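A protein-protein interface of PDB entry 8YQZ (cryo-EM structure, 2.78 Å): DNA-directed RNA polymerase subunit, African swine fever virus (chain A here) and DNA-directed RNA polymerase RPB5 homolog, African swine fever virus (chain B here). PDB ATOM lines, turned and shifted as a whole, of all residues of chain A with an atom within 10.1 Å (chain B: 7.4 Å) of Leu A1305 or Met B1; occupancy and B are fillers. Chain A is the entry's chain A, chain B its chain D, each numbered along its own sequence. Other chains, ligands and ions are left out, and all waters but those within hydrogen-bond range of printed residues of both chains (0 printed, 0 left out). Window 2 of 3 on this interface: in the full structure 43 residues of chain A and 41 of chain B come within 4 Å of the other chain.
Printed residues of chain B that touch a printed residue of chain A: Met B1, Ala B2, Lys B5, His B124, Cys B127 and Ile B128. Printed residues of chain A that touch a printed residue of chain B: Phe A1301, Met A1304, Leu A1305, Pro A1311, Tyr A1312 and Leu A1325. Hydrophobic or aromatic side chains of chain A that line the printed part of chain B: Phe A1301, Met A1304, Leu A1305, Tyr A1312 and Leu A1325. Among the printed residues, no Asp or Glu carboxylate lies within 4 Å of a Lys or Arg side-chain nitrogen of the other chain.
CD1 of Phe A1301 touches CB of His B124, 3.5 Å away. CE1 of Phe A1301 touches SG of Cys B127, 3.8 Å away. Lys B5 touches Met A1304. Ile B128 touches Met A1304 (CD1 to SD, 3.8 Å). Leu A1305 touches Met B1. Leu A1305 touches Ala B2. CG of Lys B5 touches CD2 of Leu A1305, 3.6 Å away. Ile B128 touches Pro A1311 (CD1 to O, 3.3 Å). CG1 of Ile B128 touches CE1 of Tyr A1312 (3.7 Å). Leu A1325 touches His B124 (CD1 to CB, 3.9 Å).
The backbone carbonyl oxygen (O) of Lys B5 lies within hydrogen-bond range of the side-chain hydroxyl (OG1) of Thr B8 (3.0 Å).
Printed residues of chain B within 4 Å of Met A1304: Lys B5 (3.6 Å) and Ile B128 (3.8 Å). Of chain B, only Met B1, Ala B2 and Lys B5 come within 4 Å of Leu A1305. Asp A1310 touches none of the printed residues of chain B. Printed residues of chain B within 4 Å of Tyr A1312: Ile B128 (3.7 Å). Of chain A, only Leu A1305 (3.7 Å) comes within 4 Å of Met B1. Printed residues of chain A within 4 Å of Lys B5: Met A1304 and Leu A1305. Of the printed residues of chain A, His B124 touches Phe A1301 (3.5 Å) and Leu A1325 (3.9 Å). The nearest residue of chain B that does not touch Leu A1305 is Cys B127 (4.5 Å). The nearest residue of chain A that does not touch Met B1 is Asp A1307 (4.1 Å). The nearest printed residue of chain A that does not touch Cys B127 is Met A1304 (4.5 Å).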
ATOM      1  N   MET A1094      -9.606  25.486  16.928  1.00  0.00           N
ATOM      2  CA  MET A1094      -8.437  24.949  16.251  1.00  0.00           C
ATOM      3  C   MET A1094      -8.191  25.818  15.033  1.00  0.00           C
ATOM      4  O   MET A1094      -9.064  26.573  14.613  1.00  0.00           O
ATOM      5  CB  MET A1094      -8.635  23.489  15.864  1.00  0.00           C
ATOM      6  CG  MET A1094      -7.879  22.515  16.714  1.00  0.00           C
ATOM      7  SD  MET A1094      -8.400  20.813  16.478  1.00  0.00           S
ATOM      8  CE  MET A1094      -7.909  20.534  14.792  1.00  0.00           C
ATOM      9  N   LEU A1096      -6.215  25.251  11.325  1.00  0.00           N
ATOM     10  CA  LEU A1096      -5.547  24.272  10.479  1.00  0.00           C
ATOM     11  C   LEU A1096      -5.014  24.942   9.221  1.00  0.00           C
ATOM     12  O   LEU A1096      -5.674  25.806   8.642  1.00  0.00           O
ATOM     13  CB  LEU A1096      -6.507  23.142  10.123  1.00  0.00           C
ATOM     14  CG  LEU A1096      -7.021  22.404  11.353  1.00  0.00           C
ATOM     15  CD1 LEU A1096      -8.395  21.831  11.123  1.00  0.00           C
ATOM     16  CD2 LEU A1096      -6.046  21.319  11.748  1.00  0.00           C
ATOM     17  N   LYS A1099      -2.260  21.843   3.118  1.00  0.00           N
ATOM     18  CA  LYS A1099      -1.107  20.968   2.956  1.00  0.00           C
ATOM     19  C   LYS A1099      -0.019  21.543   2.059  1.00  0.00           C
ATOM     20  O   LYS A1099       1.093  21.005   2.051  1.00  0.00           O
ATOM     21  CB  LYS A1099      -1.564  19.616   2.417  1.00  0.00           C
ATOM     22  CG  LYS A1099      -0.653  18.449   2.743  1.00  0.00           C
ATOM     23  CD  LYS A1099       0.084  18.631   4.054  1.00  0.00           C
ATOM     24  CE  LYS A1099       0.823  17.368   4.441  1.00  0.00           C
ATOM     25  NZ  LYS A1099      -0.098  16.214   4.566  1.00  0.00           N
ATOM     26  N   SER A1116     -15.161  18.952   4.217  1.00  0.00           N
ATOM     27  CA  SER A1116     -14.771  17.550   4.283  1.00  0.00           C
ATOM     28  C   SER A1116     -14.590  17.077   5.717  1.00  0.00           C
ATOM     29  O   SER A1116     -14.876  15.916   6.033  1.00  0.00           O
ATOM     30  CB  SER A1116     -13.481  17.338   3.494  1.00  0.00           C
ATOM     31  OG  SER A1116     -12.740  16.267   4.039  1.00  0.00           O
ATOM     32  N   ILE A1117     -14.092  17.952   6.595  1.00  0.00           N
ATOM     33  CA  ILE A1117     -13.679  17.522   7.926  1.00  0.00           C
ATOM     34  C   ILE A1117     -14.747  17.734   8.989  1.00  0.00           C
ATOM     35  O   ILE A1117     -14.594  17.231  10.105  1.00  0.00           O
ATOM     36  CB  ILE A1117     -12.381  18.236   8.332  1.00  0.00           C
ATOM     37  CG1 ILE A1117     -12.662  19.689   8.711  1.00  0.00           C
ATOM     38  CG2 ILE A1117     -11.358  18.161   7.212  1.00  0.00           C
ATOM     39  CD1 ILE A1117     -11.432  20.523   8.792  1.00  0.00           C
ATOM     40  N   GLY A1261     -15.998  13.271   8.332  1.00  0.00           N
ATOM     41  CA  GLY A1261     -15.375  14.339   9.079  1.00  0.00           C
ATOM     42  C   GLY A1261     -14.467  13.802  10.159  1.00  0.00           C
ATOM     43  O   GLY A1261     -14.007  12.658  10.113  1.00  0.00           O
ATOM     44  N   ILE A1262     -14.193  14.643  11.144  1.00  0.00           N
ATOM     45  CA  ILE A1262     -13.362  14.303  12.296  1.00  0.00           C
ATOM     46  C   ILE A1262     -14.199  14.503  13.549  1.00  0.00           C
ATOM     47  O   ILE A1262     -14.811  15.564  13.703  1.00  0.00           O
ATOM     48  CB  ILE A1262     -12.086  15.166  12.356  1.00  0.00           C
ATOM     49  CG1 ILE A1262     -11.231  14.963  11.107  1.00  0.00           C
ATOM     50  CG2 ILE A1262     -11.279  14.846  13.594  1.00  0.00           C
ATOM     51  CD1 ILE A1262     -10.234  16.063  10.873  1.00  0.00           C
ATOM     52  N   PRO A1263     -14.261  13.529  14.455  1.00  0.00           N
ATOM     53  CA  PRO A1263     -15.106  13.685  15.644  1.00  0.00           C
ATOM     54  C   PRO A1263     -14.674  14.875  16.485  1.00  0.00           C
ATOM     55  O   PRO A1263     -13.488  15.187  16.593  1.00  0.00           O
ATOM     56  CB  PRO A1263     -14.904  12.366  16.398  1.00  0.00           C
ATOM     57  CG  PRO A1263     -14.392  11.420  15.389  1.00  0.00           C
ATOM     58  CD  PRO A1263     -13.584  12.227  14.430  1.00  0.00           C
ATOM     59  N   ILE A1265     -15.384  17.982  15.801  1.00  0.00           N
ATOM     60  CA  ILE A1265     -15.363  19.201  14.994  1.00  0.00           C
ATOM     61  C   ILE A1265     -16.808  19.481  14.593  1.00  0.00           C
ATOM     62  O   ILE A1265     -17.420  18.744  13.829  1.00  0.00           O
ATOM     63  CB  ILE A1265     -14.427  19.082  13.796  1.00  0.00           C
ATOM     64  CG1 ILE A1265     -12.990  19.368  14.229  1.00  0.00           C
ATOM     65  CG2 ILE A1265     -14.811  20.055  12.720  1.00  0.00           C
ATOM     66  CD1 ILE A1265     -11.944  18.544  13.525  1.00  0.00           C
ATOM     67  N   ASN A1299      -9.670  18.598  18.129  1.00  0.00           N
ATOM     68  CA  ASN A1299      -9.206  17.214  18.037  1.00  0.00           C
ATOM     69  C   ASN A1299      -7.892  17.243  17.258  1.00  0.00           C
ATOM     70  O   ASN A1299      -7.888  17.200  16.028  1.00  0.00           O
ATOM     71  CB  ASN A1299     -10.237  16.320  17.374  1.00  0.00           C
ATOM     72  CG  ASN A1299     -10.038  14.864  17.702  1.00  0.00           C
ATOM     73  OD1 ASN A1299      -9.157  14.211  17.152  1.00  0.00           O
ATOM     74  ND2 ASN A1299     -10.860  14.342  18.597  1.00  0.00           N
ATOM     75  N   ILE A1300      -6.780  17.318  17.991  1.00  0.00           N
ATOM     76  CA  ILE A1300      -5.481  17.417  17.336  1.00  0.00           C
ATOM     77  C   ILE A1300      -5.122  16.101  16.663  1.00  0.00           C
ATOM     78  O   ILE A1300      -4.617  16.086  15.539  1.00  0.00           O
ATOM     79  CB  ILE A1300      -4.397  17.855  18.339  1.00  0.00           C
ATOM     80  CG1 ILE A1300      -4.558  19.329  18.691  1.00  0.00           C
ATOM     81  CG2 ILE A1300      -3.018  17.658  17.755  1.00  0.00           C
ATOM     82  CD1 ILE A1300      -3.640  19.789  19.785  1.00  0.00           C
ATOM     83  N   PHE A1301      -5.379  14.978  17.338  1.00  0.00           N
ATOM     84  CA  PHE A1301      -5.018  13.677  16.785  1.00  0.00           C
ATOM     85  C   PHE A1301      -5.797  13.362  15.518  1.00  0.00           C
ATOM     86  O   PHE A1301      -5.231  12.816  14.567  1.00  0.00           O
ATOM     87  CB  PHE A1301      -5.228  12.589  17.836  1.00  0.00           C
ATOM     88  CG  PHE A1301      -4.946  11.203  17.346  1.00  0.00           C
ATOM     89  CD1 PHE A1301      -3.831  10.934  16.576  1.00  0.00           C
ATOM     90  CD2 PHE A1301      -5.779  10.160  17.686  1.00  0.00           C
ATOM     91  CE1 PHE A1301      -3.568   9.657  16.132  1.00  0.00           C
ATOM     92  CE2 PHE A1301      -5.516   8.882  17.251  1.00  0.00           C
ATOM     93  CZ  PHE A1301      -4.410   8.630  16.474  1.00  0.00           C
ATOM     94  N   GLY A1302      -7.085  13.699  15.481  1.00  0.00           N
ATOM     95  CA  GLY A1302      -7.857  13.488  14.271  1.00  0.00           C
ATOM     96  C   GLY A1302      -7.350  14.303  13.098  1.00  0.00           C
ATOM     97  O   GLY A1302      -7.351  13.834  11.961  1.00  0.00           O
ATOM     98  N   ALA A1303      -6.903  15.530  13.354  1.00  0.00           N
ATOM     99  CA  ALA A1303      -6.440  16.387  12.272  1.00  0.00           C
ATOM    100  C   ALA A1303      -5.128  15.917  11.656  1.00  0.00           C
ATOM    101  O   ALA A1303      -4.862  16.243  10.497  1.00  0.00           O
ATOM    102  CB  ALA A1303      -6.296  17.827  12.756  1.00  0.00           C
ATOM    103  N   MET A1304      -4.280  15.202  12.396  1.00  0.00           N
ATOM    104  CA  MET A1304      -3.098  14.646  11.748  1.00  0.00           C
ATOM    105  C   MET A1304      -3.429  13.383  10.969  1.00  0.00           C
ATOM    106  O   MET A1304      -2.627  12.946  10.136  1.00  0.00           O
ATOM    107  CB  MET A1304      -1.983  14.367  12.756  1.00  0.00           C
ATOM    108  CG  MET A1304      -2.146  15.007  14.105  1.00  0.00           C
ATOM    109  SD  MET A1304      -0.782  14.611  15.219  1.00  0.00           S
ATOM    110  CE  MET A1304      -1.272  13.023  15.857  1.00  0.00           C
ATOM    111  N   LEU A1305      -4.591  12.784  11.230  1.00  0.00           N
ATOM    112  CA  LEU A1305      -5.104  11.707  10.395  1.00  0.00           C
ATOM    113  C   LEU A1305      -5.927  12.292   9.257  1.00  0.00           C
ATOM    114  O   LEU A1305      -7.096  11.938   9.077  1.00  0.00           O
ATOM    115  CB  LEU A1305      -5.945  10.736  11.217  1.00  0.00           C
ATOM    116  CG  LEU A1305      -5.282  10.150  12.455  1.00  0.00           C
ATOM    117  CD1 LEU A1305      -6.223   9.175  13.128  1.00  0.00           C
ATOM    118  CD2 LEU A1305      -3.968   9.490  12.101  1.00  0.00           C
ATOM    119  N   ASP A1306      -5.328  13.206   8.502  1.00  0.00           N
ATOM    120  CA  ASP A1306      -5.989  13.843   7.373  1.00  0.00           C
ATOM    121  C   ASP A1306      -4.946  14.440   6.445  1.00  0.00           C
ATOM    122  O   ASP A1306      -4.099  15.227   6.877  1.00  0.00           O
ATOM    123  CB  ASP A1306      -6.972  14.913   7.843  1.00  0.00           C
ATOM    124  CG  ASP A1306      -7.861  15.417   6.722  1.00  0.00           C
ATOM    125  OD1 ASP A1306      -7.711  14.944   5.576  1.00  0.00           O
ATOM    126  OD2 ASP A1306      -8.715  16.285   6.981  1.00  0.00           O
ATOM    127  N   ASP A1307      -4.997  14.071   5.170  1.00  0.00           N
ATOM    128  CA  ASP A1307      -3.983  14.476   4.213  1.00  0.00           C
ATOM    129  C   ASP A1307      -4.180  15.890   3.692  1.00  0.00           C
ATOM    130  O   ASP A1307      -3.255  16.444   3.090  1.00  0.00           O
ATOM    131  CB  ASP A1307      -3.967  13.506   3.034  1.00  0.00           C
ATOM    132  CG  ASP A1307      -3.950  12.064   3.475  1.00  0.00           C
ATOM    133  OD1 ASP A1307      -4.609  11.745   4.487  1.00  0.00           O
ATOM    134  OD2 ASP A1307      -3.282  11.244   2.809  1.00  0.00           O
ATOM    135  N   ASN A1308      -5.348  16.487   3.907  1.00  0.00           N
ATOM    136  CA  ASN A1308      -5.604  17.827   3.405  1.00  0.00           C
ATOM    137  C   ASN A1308      -5.084  18.915   4.328  1.00  0.00           C
ATOM    138  O   ASN A1308      -5.124  20.091   3.958  1.00  0.00           O
ATOM    139  CB  ASN A1308      -7.103  18.025   3.180  1.00  0.00           C
ATOM    140  CG  ASN A1308      -7.693  16.991   2.244  1.00  0.00           C
ATOM    141  OD1 ASN A1308      -8.631  16.279   2.599  1.00  0.00           O
ATOM    142  ND2 ASN A1308      -7.135  16.896   1.042  1.00  0.00           N
ATOM    143  N   ILE A1309      -4.586  18.554   5.504  1.00  0.00           N
ATOM    144  CA  ILE A1309      -4.129  19.502   6.506  1.00  0.00           C
ATOM    145  C   ILE A1309      -2.655  19.253   6.777  1.00  0.00           C
ATOM    146  O   ILE A1309      -2.220  18.100   6.847  1.00  0.00           O
ATOM    147  CB  ILE A1309      -4.959  19.379   7.799  1.00  0.00           C
ATOM    148  CG1 ILE A1309      -6.354  19.966   7.594  1.00  0.00           C
ATOM    149  CG2 ILE A1309      -4.250  20.041   8.952  1.00  0.00           C
ATOM    150  CD1 ILE A1309      -7.437  19.168   8.252  1.00  0.00           C
ATOM    151  N   ASP A1310      -1.890  20.329   6.911  1.00  0.00           N
ATOM    152  CA  ASP A1310      -0.492  20.211   7.302  1.00  0.00           C
ATOM    153  C   ASP A1310      -0.419  19.819   8.768  1.00  0.00           C
ATOM    154  O   ASP A1310      -0.852  20.596   9.629  1.00  0.00           O
ATOM    155  CB  ASP A1310       0.239  21.523   7.065  1.00  0.00           C
ATOM    156  CG  ASP A1310       1.733  21.378   7.183  1.00  0.00           C
ATOM    157  OD1 ASP A1310       2.303  20.557   6.440  1.00  0.00           O
ATOM    158  OD2 ASP A1310       2.348  22.096   7.994  1.00  0.00           O
ATOM    159  N   PRO A1311       0.118  18.643   9.102  1.00  0.00           N
ATOM    160  CA  PRO A1311       0.030  18.152  10.482  1.00  0.00           C
ATOM    161  C   PRO A1311       1.103  18.697  11.406  1.00  0.00           C
ATOM    162  O   PRO A1311       1.068  18.400  12.605  1.00  0.00           O
ATOM    163  CB  PRO A1311       0.176  16.638  10.308  1.00  0.00           C
ATOM    164  CG  PRO A1311       1.065  16.511   9.133  1.00  0.00           C
ATOM    165  CD  PRO A1311       0.757  17.661   8.213  1.00  0.00           C
ATOM    166  N   TYR A1312       2.048  19.470  10.893  1.00  0.00           N
ATOM    167  CA  TYR A1312       3.129  20.036  11.681  1.00  0.00           C
ATOM    168  C   TYR A1312       2.833  21.445  12.165  1.00  0.00           C
ATOM    169  O   TYR A1312       3.721  22.083  12.730  1.00  0.00           O
ATOM    170  CB  TYR A1312       4.413  20.041  10.853  1.00  0.00           C
ATOM    171  CG  TYR A1312       4.945  18.664  10.564  1.00  0.00           C
ATOM    172  CD1 TYR A1312       5.185  17.761  11.586  1.00  0.00           C
ATOM    173  CD2 TYR A1312       5.151  18.243   9.262  1.00  0.00           C
ATOM    174  CE1 TYR A1312       5.658  16.497  11.321  1.00  0.00           C
ATOM    175  CE2 TYR A1312       5.614  16.980   8.987  1.00  0.00           C
ATOM    176  CZ  TYR A1312       5.868  16.110  10.018  1.00  0.00           C
ATOM    177  OH  TYR A1312       6.330  14.848   9.743  1.00  0.00           O
ATOM    178  N   ILE A1314      -0.531  22.459  13.445  1.00  0.00           N
ATOM    179  CA  ILE A1314      -1.865  22.486  14.034  1.00  0.00           C
ATOM    180  C   ILE A1314      -1.831  23.332  15.299  1.00  0.00           C
ATOM    181  O   ILE A1314      -1.002  23.108  16.185  1.00  0.00           O
ATOM    182  CB  ILE A1314      -2.367  21.069  14.337  1.00  0.00           C
ATOM    183  CG1 ILE A1314      -2.516  20.268  13.050  1.00  0.00           C
ATOM    184  CG2 ILE A1314      -3.685  21.128  15.074  1.00  0.00           C
ATOM    185  CD1 ILE A1314      -2.634  18.785  13.275  1.00  0.00           C
ATOM    186  N   LEU A1325      -0.920  15.656  23.528  1.00  0.00           N
ATOM    187  CA  LEU A1325      -0.363  15.340  22.225  1.00  0.00           C
ATOM    188  C   LEU A1325       1.095  15.754  22.085  1.00  0.00           C
ATOM    189  O   LEU A1325       1.843  15.118  21.341  1.00  0.00           O
ATOM    190  CB  LEU A1325      -1.192  16.017  21.131  1.00  0.00           C
ATOM    191  CG  LEU A1325      -2.146  15.158  20.299  1.00  0.00           C
ATOM    192  CD1 LEU A1325      -1.385  14.099  19.534  1.00  0.00           C
ATOM    193  CD2 LEU A1325      -3.196  14.532  21.177  1.00  0.00           C
ATOM    194  N   MET B   1      -7.110   6.135   9.952  1.00  0.00           N
ATOM    195  CA  MET B   1      -5.899   6.449   9.210  1.00  0.00           C
ATOM    196  C   MET B   1      -4.713   6.086  10.092  1.00  0.00           C
ATOM    197  O   MET B   1      -3.565   6.097   9.660  1.00  0.00           O
ATOM    198  CB  MET B   1      -5.878   7.932   8.822  1.00  0.00           C
ATOM    199  CG  MET B   1      -4.666   8.399   8.020  1.00  0.00           C
ATOM    200  SD  MET B   1      -4.050   7.147   6.883  1.00  0.00           S
ATOM    201  CE  MET B   1      -3.116   8.138   5.724  1.00  0.00           C
ATOM    202  N   ALA B   2      -5.015   5.723  11.339  1.00  0.00           N
ATOM    203  CA  ALA B   2      -3.963   5.536  12.330  1.00  0.00           C
ATOM    204  C   ALA B   2      -2.986   4.446  11.914  1.00  0.00           C
ATOM    205  O   ALA B   2      -1.787   4.542  12.192  1.00  0.00           O
ATOM    206  CB  ALA B   2      -4.576   5.218  13.691  1.00  0.00           C
ATOM    207  N   MET B   3      -3.473   3.403  11.245  1.00  0.00           N
ATOM    208  CA  MET B   3      -2.595   2.298  10.880  1.00  0.00           C
ATOM    209  C   MET B   3      -1.610   2.699   9.788  1.00  0.00           C
ATOM    210  O   MET B   3      -0.429   2.340   9.849  1.00  0.00           O
ATOM    211  CB  MET B   3      -3.427   1.093  10.457  1.00  0.00           C
ATOM    212  CG  MET B   3      -3.634   0.097  11.578  1.00  0.00           C
ATOM    213  SD  MET B   3      -2.086  -0.352  12.379  1.00  0.00           S
ATOM    214  CE  MET B   3      -2.675  -1.036  13.921  1.00  0.00           C
ATOM    215  N   GLN B   4      -2.063   3.451   8.788  1.00  0.00           N
ATOM    216  CA  GLN B   4      -1.142   3.894   7.747  1.00  0.00           C
ATOM    217  C   GLN B   4      -0.130   4.898   8.286  1.00  0.00           C
ATOM    218  O   GLN B   4       1.046   4.862   7.909  1.00  0.00           O
ATOM    219  CB  GLN B   4      -1.919   4.482   6.567  1.00  0.00           C
ATOM    220  CG  GLN B   4      -1.110   5.014   5.351  1.00  0.00           C
ATOM    221  CD  GLN B   4       0.037   4.123   4.838  1.00  0.00           C
ATOM    222  OE1 GLN B   4       0.735   3.449   5.592  1.00  0.00           O
ATOM    223  NE2 GLN B   4       0.221   4.129   3.526  1.00  0.00           N
ATOM    224  N   LYS B   5      -0.565   5.806   9.163  1.00  0.00           N
ATOM    225  CA  LYS B   5       0.374   6.741   9.779  1.00  0.00           C
ATOM    226  C   LYS B   5       1.395   6.008  10.642  1.00  0.00           C
ATOM    227  O   LYS B   5       2.586   6.343  10.625  1.00  0.00           O
ATOM    228  CB  LYS B   5      -0.383   7.777  10.601  1.00  0.00           C
ATOM    229  CG  LYS B   5      -1.268   8.691   9.786  1.00  0.00           C
ATOM    230  CD  LYS B   5      -0.456   9.469   8.786  1.00  0.00           C
ATOM    231  CE  LYS B   5      -1.327  10.388   7.963  1.00  0.00           C
ATOM    232  NZ  LYS B   5      -0.534  11.108   6.941  1.00  0.00           N
ATOM    233  N   LEU B   6       0.941   5.010  11.400  1.00  0.00           N
ATOM    234  CA  LEU B   6       1.855   4.183  12.173  1.00  0.00           C
ATOM    235  C   LEU B   6       2.874   3.513  11.271  1.00  0.00           C
ATOM    236  O   LEU B   6       4.069   3.504  11.572  1.00  0.00           O
ATOM    237  CB  LEU B   6       1.085   3.126  12.957  1.00  0.00           C
ATOM    238  CG  LEU B   6       0.632   3.422  14.379  1.00  0.00           C
ATOM    239  CD1 LEU B   6      -0.328   2.352  14.846  1.00  0.00           C
ATOM    240  CD2 LEU B   6       1.829   3.483  15.286  1.00  0.00           C
ATOM    241  N   PHE B   7       2.422   2.963  10.144  1.00  0.00           N
ATOM    242  CA  PHE B   7       3.313   2.187   9.292  1.00  0.00           C
ATOM    243  C   PHE B   7       4.509   2.987   8.794  1.00  0.00           C
ATOM    244  O   PHE B   7       5.542   2.393   8.482  1.00  0.00           O
ATOM    245  CB  PHE B   7       2.545   1.623   8.098  1.00  0.00           C
ATOM    246  CG  PHE B   7       3.371   0.737   7.219  1.00  0.00           C
ATOM    247  CD1 PHE B   7       3.732  -0.527   7.635  1.00  0.00           C
ATOM    248  CD2 PHE B   7       3.823   1.187   5.996  1.00  0.00           C
ATOM    249  CE1 PHE B   7       4.505  -1.330   6.836  1.00  0.00           C
ATOM    250  CE2 PHE B   7       4.598   0.386   5.198  1.00  0.00           C
ATOM    251  CZ  PHE B   7       4.938  -0.872   5.619  1.00  0.00           C
ATOM    252  N   THR B   8       4.412   4.310   8.715  1.00  0.00           N
ATOM    253  CA  THR B   8       5.546   5.127   8.304  1.00  0.00           C
ATOM    254  C   THR B   8       6.310   5.688   9.496  1.00  0.00           C
ATOM    255  O   THR B   8       7.553   5.637   9.557  1.00  0.00           O
ATOM    256  CB  THR B   8       5.071   6.282   7.411  1.00  0.00           C
ATOM    257  OG1 THR B   8       3.803   6.754   7.873  1.00  0.00           O
ATOM    258  CG2 THR B   8       4.931   5.827   5.975  1.00  0.00           C
ATOM    259  N   TYR B  28       2.760  -2.361   3.091  1.00  0.00           N
ATOM    260  CA  TYR B  28       1.698  -1.954   4.004  1.00  0.00           C
ATOM    261  C   TYR B  28       0.546  -2.948   3.994  1.00  0.00           C
ATOM    262  O   TYR B  28      -0.033  -3.253   5.044  1.00  0.00           O
ATOM    263  CB  TYR B  28       1.200  -0.556   3.639  1.00  0.00           C
ATOM    264  CG  TYR B  28      -0.087  -0.184   4.323  1.00  0.00           C
ATOM    265  CD1 TYR B  28      -0.167  -0.127   5.707  1.00  0.00           C
ATOM    266  CD2 TYR B  28      -1.232   0.090   3.592  1.00  0.00           C
ATOM    267  CE1 TYR B  28      -1.344   0.200   6.337  1.00  0.00           C
ATOM    268  CE2 TYR B  28      -2.413   0.421   4.218  1.00  0.00           C
ATOM    269  CZ  TYR B  28      -2.462   0.472   5.589  1.00  0.00           C
ATOM    270  OH  TYR B  28      -3.638   0.798   6.220  1.00  0.00           O
ATOM    271  N   HIS B 124      -1.447   7.860  19.244  1.00  0.00           N
ATOM    272  CA  HIS B 124      -1.120   9.197  18.759  1.00  0.00           C
ATOM    273  C   HIS B 124       0.341   9.547  18.962  1.00  0.00           C
ATOM    274  O   HIS B 124       0.833  10.488  18.336  1.00  0.00           O
ATOM    275  CB  HIS B 124      -1.997  10.249  19.436  1.00  0.00           C
ATOM    276  CG  HIS B 124      -1.900  10.263  20.929  1.00  0.00           C
ATOM    277  ND1 HIS B 124      -0.768  10.673  21.599  1.00  0.00           N
ATOM    278  CD2 HIS B 124      -2.806   9.950  21.883  1.00  0.00           C
ATOM    279  CE1 HIS B 124      -0.973  10.588  22.900  1.00  0.00           C
ATOM    280  NE2 HIS B 124      -2.203  10.153  23.099  1.00  0.00           N
ATOM    281  N   CYS B 127       2.008   8.571  15.477  1.00  0.00           N
ATOM    282  CA  CYS B 127       1.317   8.869  14.233  1.00  0.00           C
ATOM    283  C   CYS B 127       1.795  10.162  13.599  1.00  0.00           C
ATOM    284  O   CYS B 127       1.076  10.742  12.783  1.00  0.00           O
ATOM    285  CB  CYS B 127      -0.191   8.921  14.461  1.00  0.00           C
ATOM    286  SG  CYS B 127      -0.945   7.315  14.762  1.00  0.00           S
ATOM    287  N   ILE B 128       2.986  10.632  13.970  1.00  0.00           N
ATOM    288  CA  ILE B 128       3.565  11.841  13.400  1.00  0.00           C
ATOM    289  C   ILE B 128       5.041  11.844  13.753  1.00  0.00           C
ATOM    290  O   ILE B 128       5.471  11.151  14.676  1.00  0.00           O
ATOM    291  CB  ILE B 128       2.834  13.104  13.920  1.00  0.00           C
ATOM    292  CG1 ILE B 128       3.220  14.336  13.111  1.00  0.00           C
ATOM    293  CG2 ILE B 128       3.097  13.303  15.390  1.00  0.00           C
ATOM    294  CD1 ILE B 128       2.475  15.564  13.527  1.00  0.00           C
